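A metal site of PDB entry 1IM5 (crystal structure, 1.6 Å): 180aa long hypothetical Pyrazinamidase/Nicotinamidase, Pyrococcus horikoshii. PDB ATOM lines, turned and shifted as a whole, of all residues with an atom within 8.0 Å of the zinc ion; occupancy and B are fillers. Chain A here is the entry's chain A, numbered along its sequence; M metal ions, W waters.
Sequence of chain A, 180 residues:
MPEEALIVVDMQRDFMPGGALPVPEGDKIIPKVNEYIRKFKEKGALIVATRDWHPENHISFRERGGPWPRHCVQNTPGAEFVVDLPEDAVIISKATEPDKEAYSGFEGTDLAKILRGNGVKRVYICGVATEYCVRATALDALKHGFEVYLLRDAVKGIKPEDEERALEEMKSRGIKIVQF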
ATOM      1  N   ASP A  10       4.963 -23.756 -20.172  1.00  0.00           N
ATOM      2  CA  ASP A  10       4.543 -22.876 -19.087  1.00  0.00           C
ATOM      3  C   ASP A  10       3.137 -23.101 -18.584  1.00  0.00           C
ATOM      4  O   ASP A  10       2.365 -22.167 -18.303  1.00  0.00           O
ATOM      5  CB  ASP A  10       4.774 -21.433 -19.583  1.00  0.00           C
ATOM      6  CG  ASP A  10       6.260 -21.181 -19.787  1.00  0.00           C
ATOM      7  OD1 ASP A  10       7.097 -22.093 -19.526  1.00  0.00           O
ATOM      8  OD2 ASP A  10       6.625 -20.043 -20.189  1.00  0.00           O
ATOM      9  N   GLN A  12       1.549 -23.404 -15.890  1.00  0.00           N
ATOM     10  CA  GLN A  12       1.759 -23.075 -14.487  1.00  0.00           C
ATOM     11  C   GLN A  12       0.589 -22.280 -13.900  1.00  0.00           C
ATOM     12  O   GLN A  12      -0.099 -21.584 -14.659  1.00  0.00           O
ATOM     13  CB  GLN A  12       3.039 -22.254 -14.403  1.00  0.00           C
ATOM     14  CG  GLN A  12       4.280 -23.079 -14.763  1.00  0.00           C
ATOM     15  CD  GLN A  12       5.459 -22.105 -14.886  1.00  0.00           C
ATOM     16  OE1 GLN A  12       5.696 -21.543 -15.949  1.00  0.00           O
ATOM     17  NE2 GLN A  12       6.155 -21.893 -13.778  1.00  0.00           N
ATOM     18  N   PHE A  15      -0.249 -18.606 -14.906  1.00  0.00           N
ATOM     19  CA  PHE A  15      -0.769 -18.345 -16.257  1.00  0.00           C
ATOM     20  C   PHE A  15      -2.165 -18.895 -16.495  1.00  0.00           C
ATOM     21  O   PHE A  15      -2.622 -18.770 -17.631  1.00  0.00           O
ATOM     22  CB  PHE A  15       0.179 -18.942 -17.298  1.00  0.00           C
ATOM     23  CG  PHE A  15       1.562 -18.318 -17.328  1.00  0.00           C
ATOM     24  CD1 PHE A  15       1.709 -16.948 -17.343  1.00  0.00           C
ATOM     25  CD2 PHE A  15       2.705 -19.115 -17.346  1.00  0.00           C
ATOM     26  CE1 PHE A  15       2.970 -16.385 -17.370  1.00  0.00           C
ATOM     27  CE2 PHE A  15       3.971 -18.557 -17.386  1.00  0.00           C
ATOM     28  CZ  PHE A  15       4.081 -17.192 -17.399  1.00  0.00           C
ATOM     29  N   LEU A  21      -0.910 -13.747 -13.918  1.00  0.00           N
ATOM     30  CA  LEU A  21      -0.785 -13.375 -15.328  1.00  0.00           C
ATOM     31  C   LEU A  21      -1.604 -14.341 -16.187  1.00  0.00           C
ATOM     32  O   LEU A  21      -1.066 -15.083 -16.991  1.00  0.00           O
ATOM     33  CB  LEU A  21       0.687 -13.337 -15.733  1.00  0.00           C
ATOM     34  CG  LEU A  21       1.061 -12.591 -17.007  1.00  0.00           C
ATOM     35  CD1 LEU A  21       0.197 -11.358 -17.186  1.00  0.00           C
ATOM     36  CD2 LEU A  21       2.536 -12.206 -17.030  1.00  0.00           C
ATOM     37  N   ARG A  51       9.120 -24.292 -17.668  1.00  0.00           N
ATOM     38  CA  ARG A  51       8.490 -23.411 -16.713  1.00  0.00           C
ATOM     39  C   ARG A  51       9.277 -22.099 -16.621  1.00  0.00           C
ATOM     40  O   ARG A  51      10.503 -22.158 -16.627  1.00  0.00           O
ATOM     41  CB  ARG A  51       8.419 -24.061 -15.332  1.00  0.00           C
ATOM     42  CG  ARG A  51       9.754 -24.418 -14.705  1.00  0.00           C
ATOM     43  CD  ARG A  51       9.550 -25.043 -13.328  1.00  0.00           C
ATOM     44  NE  ARG A  51      10.838 -25.405 -12.729  1.00  0.00           N
ATOM     45  CZ  ARG A  51      10.970 -25.971 -11.538  1.00  0.00           C
ATOM     46  NH1 ARG A  51       9.912 -26.267 -10.782  1.00  0.00           N
ATOM     47  NH2 ARG A  51      12.193 -26.261 -11.105  1.00  0.00           N
ATOM     48  N   ASP A  52       8.543 -21.017 -16.490  1.00  0.00           N
ATOM     49  CA  ASP A  52       9.100 -19.750 -16.037  1.00  0.00           C
ATOM     50  C   ASP A  52       9.521 -19.960 -14.586  1.00  0.00           C
ATOM     51  O   ASP A  52       8.726 -20.478 -13.819  1.00  0.00           O
ATOM     52  CB  ASP A  52       8.069 -18.624 -16.075  1.00  0.00           C
ATOM     53  CG  ASP A  52       8.335 -17.523 -17.053  1.00  0.00           C
ATOM     54  OD1 ASP A  52       9.296 -17.636 -17.821  1.00  0.00           O
ATOM     55  OD2 ASP A  52       7.551 -16.536 -17.064  1.00  0.00           O
ATOM     56  N   TRP A  53      10.724 -19.560 -14.225  1.00  0.00           N
ATOM     57  CA  TRP A  53      11.223 -19.850 -12.880  1.00  0.00           C
ATOM     58  C   TRP A  53      12.062 -18.648 -12.455  1.00  0.00           C
ATOM     59  O   TRP A  53      13.284 -18.703 -12.432  1.00  0.00           O
ATOM     60  CB  TRP A  53      12.011 -21.137 -12.920  1.00  0.00           C
ATOM     61  CG  TRP A  53      12.375 -21.791 -11.646  1.00  0.00           C
ATOM     62  CD1 TRP A  53      13.645 -21.972 -11.186  1.00  0.00           C
ATOM     63  CD2 TRP A  53      11.480 -22.354 -10.675  1.00  0.00           C
ATOM     64  NE1 TRP A  53      13.598 -22.633  -9.963  1.00  0.00           N
ATOM     65  CE2 TRP A  53      12.276 -22.865  -9.626  1.00  0.00           C
ATOM     66  CE3 TRP A  53      10.077 -22.452 -10.611  1.00  0.00           C
ATOM     67  CZ2 TRP A  53      11.715 -23.496  -8.500  1.00  0.00           C
ATOM     68  CZ3 TRP A  53       9.541 -23.067  -9.496  1.00  0.00           C
ATOM     69  CH2 TRP A  53      10.349 -23.588  -8.455  1.00  0.00           C
ATOM     70  N   HIS A  54      11.283 -17.613 -12.168  1.00  0.00           N
ATOM     71  CA  HIS A  54      11.831 -16.286 -11.983  1.00  0.00           C
ATOM     72  C   HIS A  54      12.273 -16.036 -10.543  1.00  0.00           C
ATOM     73  O   HIS A  54      11.636 -16.442  -9.593  1.00  0.00           O
ATOM     74  CB  HIS A  54      10.790 -15.224 -12.331  1.00  0.00           C
ATOM     75  CG  HIS A  54      10.418 -15.097 -13.761  1.00  0.00           C
ATOM     76  ND1 HIS A  54      11.321 -15.106 -14.803  1.00  0.00           N
ATOM     77  CD2 HIS A  54       9.194 -14.881 -14.313  1.00  0.00           C
ATOM     78  CE1 HIS A  54      10.666 -14.924 -15.944  1.00  0.00           C
ATOM     79  NE2 HIS A  54       9.381 -14.805 -15.666  1.00  0.00           N
ATOM     80  N   HIS A  58      12.710  -9.801 -10.730  1.00  0.00           N
ATOM     81  CA  HIS A  58      13.134 -10.096 -12.090  1.00  0.00           C
ATOM     82  C   HIS A  58      12.913  -8.886 -12.994  1.00  0.00           C
ATOM     83  O   HIS A  58      11.943  -8.135 -12.795  1.00  0.00           O
ATOM     84  CB  HIS A  58      12.385 -11.322 -12.613  1.00  0.00           C
ATOM     85  CG  HIS A  58      12.911 -11.826 -13.925  1.00  0.00           C
ATOM     86  ND1 HIS A  58      12.243 -11.651 -15.119  1.00  0.00           N
ATOM     87  CD2 HIS A  58      14.052 -12.492 -14.238  1.00  0.00           C
ATOM     88  CE1 HIS A  58      12.938 -12.190 -16.116  1.00  0.00           C
ATOM     89  NE2 HIS A  58      14.037 -12.703 -15.591  1.00  0.00           N
ATOM     90  N   SER A  60      11.840  -8.628 -15.895  1.00  0.00           N
ATOM     91  CA  SER A  60      10.588  -8.518 -16.666  1.00  0.00           C
ATOM     92  C   SER A  60       9.434  -7.979 -15.845  1.00  0.00           C
ATOM     93  O   SER A  60       8.335  -7.791 -16.387  1.00  0.00           O
ATOM     94  CB  SER A  60      10.189  -9.890 -17.236  1.00  0.00           C
ATOM     95  OG  SER A  60       9.738 -10.736 -16.172  1.00  0.00           O
ATOM     96  N   PHE A  61       9.614  -7.756 -14.545  1.00  0.00           N
ATOM     97  CA  PHE A  61       8.495  -7.394 -13.694  1.00  0.00           C
ATOM     98  C   PHE A  61       8.342  -5.875 -13.583  1.00  0.00           C
ATOM     99  O   PHE A  61       9.308  -5.127 -13.761  1.00  0.00           O
ATOM    100  CB  PHE A  61       8.638  -7.906 -12.263  1.00  0.00           C
ATOM    101  CG  PHE A  61       8.723  -9.414 -12.086  1.00  0.00           C
ATOM    102  CD1 PHE A  61       8.377 -10.293 -13.113  1.00  0.00           C
ATOM    103  CD2 PHE A  61       9.174  -9.917 -10.883  1.00  0.00           C
ATOM    104  CE1 PHE A  61       8.488 -11.663 -12.889  1.00  0.00           C
ATOM    105  CE2 PHE A  61       9.287 -11.279 -10.654  1.00  0.00           C
ATOM    106  CZ  PHE A  61       8.941 -12.159 -11.680  1.00  0.00           C
ATOM    107  N   TRP A  68       5.518  -6.997 -17.086  1.00  0.00           N
ATOM    108  CA  TRP A  68       4.538  -7.919 -16.488  1.00  0.00           C
ATOM    109  C   TRP A  68       4.412  -7.792 -14.983  1.00  0.00           C
ATOM    110  O   TRP A  68       5.370  -7.402 -14.299  1.00  0.00           O
ATOM    111  CB  TRP A  68       4.927  -9.364 -16.820  1.00  0.00           C
ATOM    112  CG  TRP A  68       5.173  -9.543 -18.299  1.00  0.00           C
ATOM    113  CD1 TRP A  68       6.330  -9.818 -18.945  1.00  0.00           C
ATOM    114  CD2 TRP A  68       4.160  -9.438 -19.307  1.00  0.00           C
ATOM    115  NE1 TRP A  68       6.114  -9.892 -20.305  1.00  0.00           N
ATOM    116  CE2 TRP A  68       4.781  -9.657 -20.550  1.00  0.00           C
ATOM    117  CE3 TRP A  68       2.786  -9.168 -19.271  1.00  0.00           C
ATOM    118  CZ2 TRP A  68       4.101  -9.633 -21.762  1.00  0.00           C
ATOM    119  CZ3 TRP A  68       2.100  -9.140 -20.471  1.00  0.00           C
ATOM    120  CH2 TRP A  68       2.764  -9.369 -21.682  1.00  0.00           C
ATOM    121  N   PRO A  69       3.258  -8.171 -14.436  1.00  0.00           N
ATOM    122  CA  PRO A  69       3.147  -8.259 -12.977  1.00  0.00           C
ATOM    123  C   PRO A  69       4.043  -9.411 -12.534  1.00  0.00           C
ATOM    124  O   PRO A  69       4.295 -10.303 -13.334  1.00  0.00           O
ATOM    125  CB  PRO A  69       1.696  -8.630 -12.717  1.00  0.00           C
ATOM    126  CG  PRO A  69       1.186  -9.165 -14.007  1.00  0.00           C
ATOM    127  CD  PRO A  69       2.009  -8.534 -15.105  1.00  0.00           C
ATOM    128  N   ARG A  70       4.495  -9.359 -11.290  1.00  0.00           N
ATOM    129  CA  ARG A  70       5.217 -10.478 -10.717  1.00  0.00           C
ATOM    130  C   ARG A  70       4.541 -11.802 -10.994  1.00  0.00           C
ATOM    131  O   ARG A  70       3.359 -11.902 -10.737  1.00  0.00           O
ATOM    132  CB  ARG A  70       5.272 -10.257  -9.209  1.00  0.00           C
ATOM    133  CG  ARG A  70       5.952 -11.359  -8.412  1.00  0.00           C
ATOM    134  CD  ARG A  70       5.911 -10.974  -6.932  1.00  0.00           C
ATOM    135  NE  ARG A  70       6.488 -11.973  -6.050  1.00  0.00           N
ATOM    136  CZ  ARG A  70       5.852 -13.044  -5.592  1.00  0.00           C
ATOM    137  NH1 ARG A  70       4.572 -13.269  -5.934  1.00  0.00           N
ATOM    138  NH2 ARG A  70       6.522 -13.869  -4.780  1.00  0.00           N
ATOM    139  N   HIS A  71       5.295 -12.803 -11.463  1.00  0.00           N
ATOM    140  CA  HIS A  71       4.663 -14.080 -11.780  1.00  0.00           C
ATOM    141  C   HIS A  71       5.720 -15.181 -11.782  1.00  0.00           C
ATOM    142  O   HIS A  71       6.893 -14.900 -11.999  1.00  0.00           O
ATOM    143  CB  HIS A  71       3.960 -14.025 -13.140  1.00  0.00           C
ATOM    144  CG  HIS A  71       4.949 -13.757 -14.247  1.00  0.00           C
ATOM    145  ND1 HIS A  71       5.395 -12.502 -14.577  1.00  0.00           N
ATOM    146  CD2 HIS A  71       5.583 -14.615 -15.085  1.00  0.00           C
ATOM    147  CE1 HIS A  71       6.254 -12.587 -15.592  1.00  0.00           C
ATOM    148  NE2 HIS A  71       6.390 -13.868 -15.898  1.00  0.00           N
ATOM    149  N   CYS A  72       5.292 -16.403 -11.515  1.00  0.00           N
ATOM    150  CA  CYS A  72       6.072 -17.624 -11.586  1.00  0.00           C
ATOM    151  C   CYS A  72       7.393 -17.510 -10.841  1.00  0.00           C
ATOM    152  O   CYS A  72       8.425 -17.893 -11.359  1.00  0.00           O
ATOM    153  CB  CYS A  72       6.318 -18.005 -13.058  1.00  0.00           C
ATOM    154  SG  CYS A  72       4.750 -18.314 -13.935  1.00  0.00           S
ATOM    155  N   VAL A  73       7.337 -16.993  -9.619  1.00  0.00           N
ATOM    156  CA  VAL A  73       8.543 -16.832  -8.796  1.00  0.00           C
ATOM    157  C   VAL A  73       8.927 -18.178  -8.185  1.00  0.00           C
ATOM    158  O   VAL A  73       8.097 -18.976  -7.727  1.00  0.00           O
ATOM    159  CB  VAL A  73       8.366 -15.772  -7.708  1.00  0.00           C
ATOM    160  CG1 VAL A  73       9.527 -15.763  -6.712  1.00  0.00           C
ATOM    161  CG2 VAL A  73       8.229 -14.383  -8.340  1.00  0.00           C
ATOM    162  N   LYS A  94      13.354 -21.782 -16.916  1.00  0.00           N
ATOM    163  CA  LYS A  94      13.965 -20.685 -17.661  1.00  0.00           C
ATOM    164  C   LYS A  94      13.819 -19.322 -16.963  1.00  0.00           C
ATOM    165  O   LYS A  94      12.998 -19.098 -16.069  1.00  0.00           O
ATOM    166  CB  LYS A  94      13.373 -20.644 -19.056  1.00  0.00           C
ATOM    167  CG  LYS A  94      11.916 -20.230 -19.124  1.00  0.00           C
ATOM    168  CD  LYS A  94      11.437 -20.590 -20.545  1.00  0.00           C
ATOM    169  CE  LYS A  94       9.901 -20.661 -20.503  1.00  0.00           C
ATOM    170  NZ  LYS A  94       9.398 -19.272 -20.424  1.00  0.00           N
ATOM    171  N   ALA A  95      14.672 -18.392 -17.397  1.00  0.00           N
ATOM    172  CA  ALA A  95      14.661 -17.017 -16.907  1.00  0.00           C
ATOM    173  C   ALA A  95      14.874 -16.932 -15.396  1.00  0.00           C
ATOM    174  O   ALA A  95      14.145 -16.215 -14.677  1.00  0.00           O
ATOM    175  CB  ALA A  95      13.379 -16.308 -17.321  1.00  0.00           C
ATOM    176  N   GLU A 101      15.930 -12.129 -19.333  1.00  0.00           N
ATOM    177  CA  GLU A 101      14.642 -12.720 -19.688  1.00  0.00           C
ATOM    178  C   GLU A 101      14.855 -13.872 -20.673  1.00  0.00           C
ATOM    179  O   GLU A 101      15.849 -13.978 -21.395  1.00  0.00           O
ATOM    180  CB  GLU A 101      13.688 -11.668 -20.249  1.00  0.00           C
ATOM    181  CG  GLU A 101      12.390 -12.170 -20.859  1.00  0.00           C
ATOM    182  CD  GLU A 101      11.396 -12.729 -19.860  1.00  0.00           C
ATOM    183  OE1 GLU A 101      11.708 -13.750 -19.222  1.00  0.00           O
ATOM    184  OE2 GLU A 101      10.277 -12.185 -19.711  1.00  0.00           O
ATOM    185  N   ALA A 102      13.882 -14.764 -20.688  1.00  0.00           N
ATOM    186  CA  ALA A 102      13.898 -15.918 -21.572  1.00  0.00           C
ATOM    187  C   ALA A 102      12.460 -16.334 -21.917  1.00  0.00           C
ATOM    188  O   ALA A 102      11.767 -16.926 -21.107  1.00  0.00           O
ATOM    189  CB  ALA A 102      14.614 -17.108 -20.956  1.00  0.00           C
ATOM    190  N   TYR A 103      12.032 -16.023 -23.131  1.00  0.00           N
ATOM    191  CA  TYR A 103      10.698 -16.398 -23.594  1.00  0.00           C
ATOM    192  C   TYR A 103      10.664 -17.847 -24.075  1.00  0.00           C
ATOM    193  O   TYR A 103       9.795 -18.646 -23.782  1.00  0.00           O
ATOM    194  CB  TYR A 103      10.319 -15.510 -24.763  1.00  0.00           C
ATOM    195  CG  TYR A 103       9.728 -14.149 -24.455  1.00  0.00           C
ATOM    196  CD1 TYR A 103       8.360 -13.992 -24.264  1.00  0.00           C
ATOM    197  CD2 TYR A 103      10.547 -13.021 -24.357  1.00  0.00           C
ATOM    198  CE1 TYR A 103       7.815 -12.748 -23.988  1.00  0.00           C
ATOM    199  CE2 TYR A 103      10.002 -11.777 -24.082  1.00  0.00           C
ATOM    200  CZ  TYR A 103       8.636 -11.641 -23.897  1.00  0.00           C
ATOM    201  OH  TYR A 103       8.107 -10.393 -23.616  1.00  0.00           O
ATOM    202  N   CYS A 133       5.418 -17.459 -25.391  1.00  0.00           N
ATOM    203  CA  CYS A 133       6.431 -18.503 -25.220  1.00  0.00           C
ATOM    204  C   CYS A 133       6.150 -19.722 -26.088  1.00  0.00           C
ATOM    205  O   CYS A 133       7.090 -20.434 -26.440  1.00  0.00           O
ATOM    206  CB  CYS A 133       6.567 -18.894 -23.742  1.00  0.00           C
ATOM    207  SG  CYS A 133       7.081 -17.605 -22.598  1.00  0.00           S
HETATM  208 ZN    ZN M   1       7.971 -14.619 -17.201  1.00  0.00          ZN
HETATM  209  O   HOH W   1       9.469 -15.357 -18.871  1.00  0.00           O
HETATM  210  O   HOH W   2       8.575 -12.644 -17.766  1.00  0.00           O
HETATM  211  O   HOH W   3       6.769 -14.735 -19.017  1.00  0.00           O
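The side-chain amino group of Lys 94 lies within salt-bridge range of the side-chain carboxylate of Asp 52. The backbone carbonyl oxygen of Asp 52 sits at hydrogen-bond distance from the side-chain amide nitrogen of Gln 12, at 2.9 Å. N of His 54 lies within hydrogen-bond range of O of Cys 72 (3.0 Å). A ring nitrogen (ND1) of His 54 sits at hydrogen-bond distance from the backbone carbonyl oxygen of Ala 95, at 3.0 Å. ND1 of His 71 lies within hydrogen-bond range of O of Pro 69.
The zinc ion is bound by the side-chain carboxylate of Asp 52 (2.0 Å), a ring nitrogen (NE2) of His 54 (2.1 Å), water W2 (2.1 Å), water W3 (2.2 Å), a ring nitrogen (NE2) of His 71 (2.2 Å) and water W1 (2.4 Å). The zinc ion has six donor atoms within binding distance.
Water W2 bridges OE2 of Glu 101 (2.6 Å) and OG of Ser 60 (2.7 Å). Water W1 lies within hydrogen-bond range of OD1 of Asp 52 and OE1 of Glu 101.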
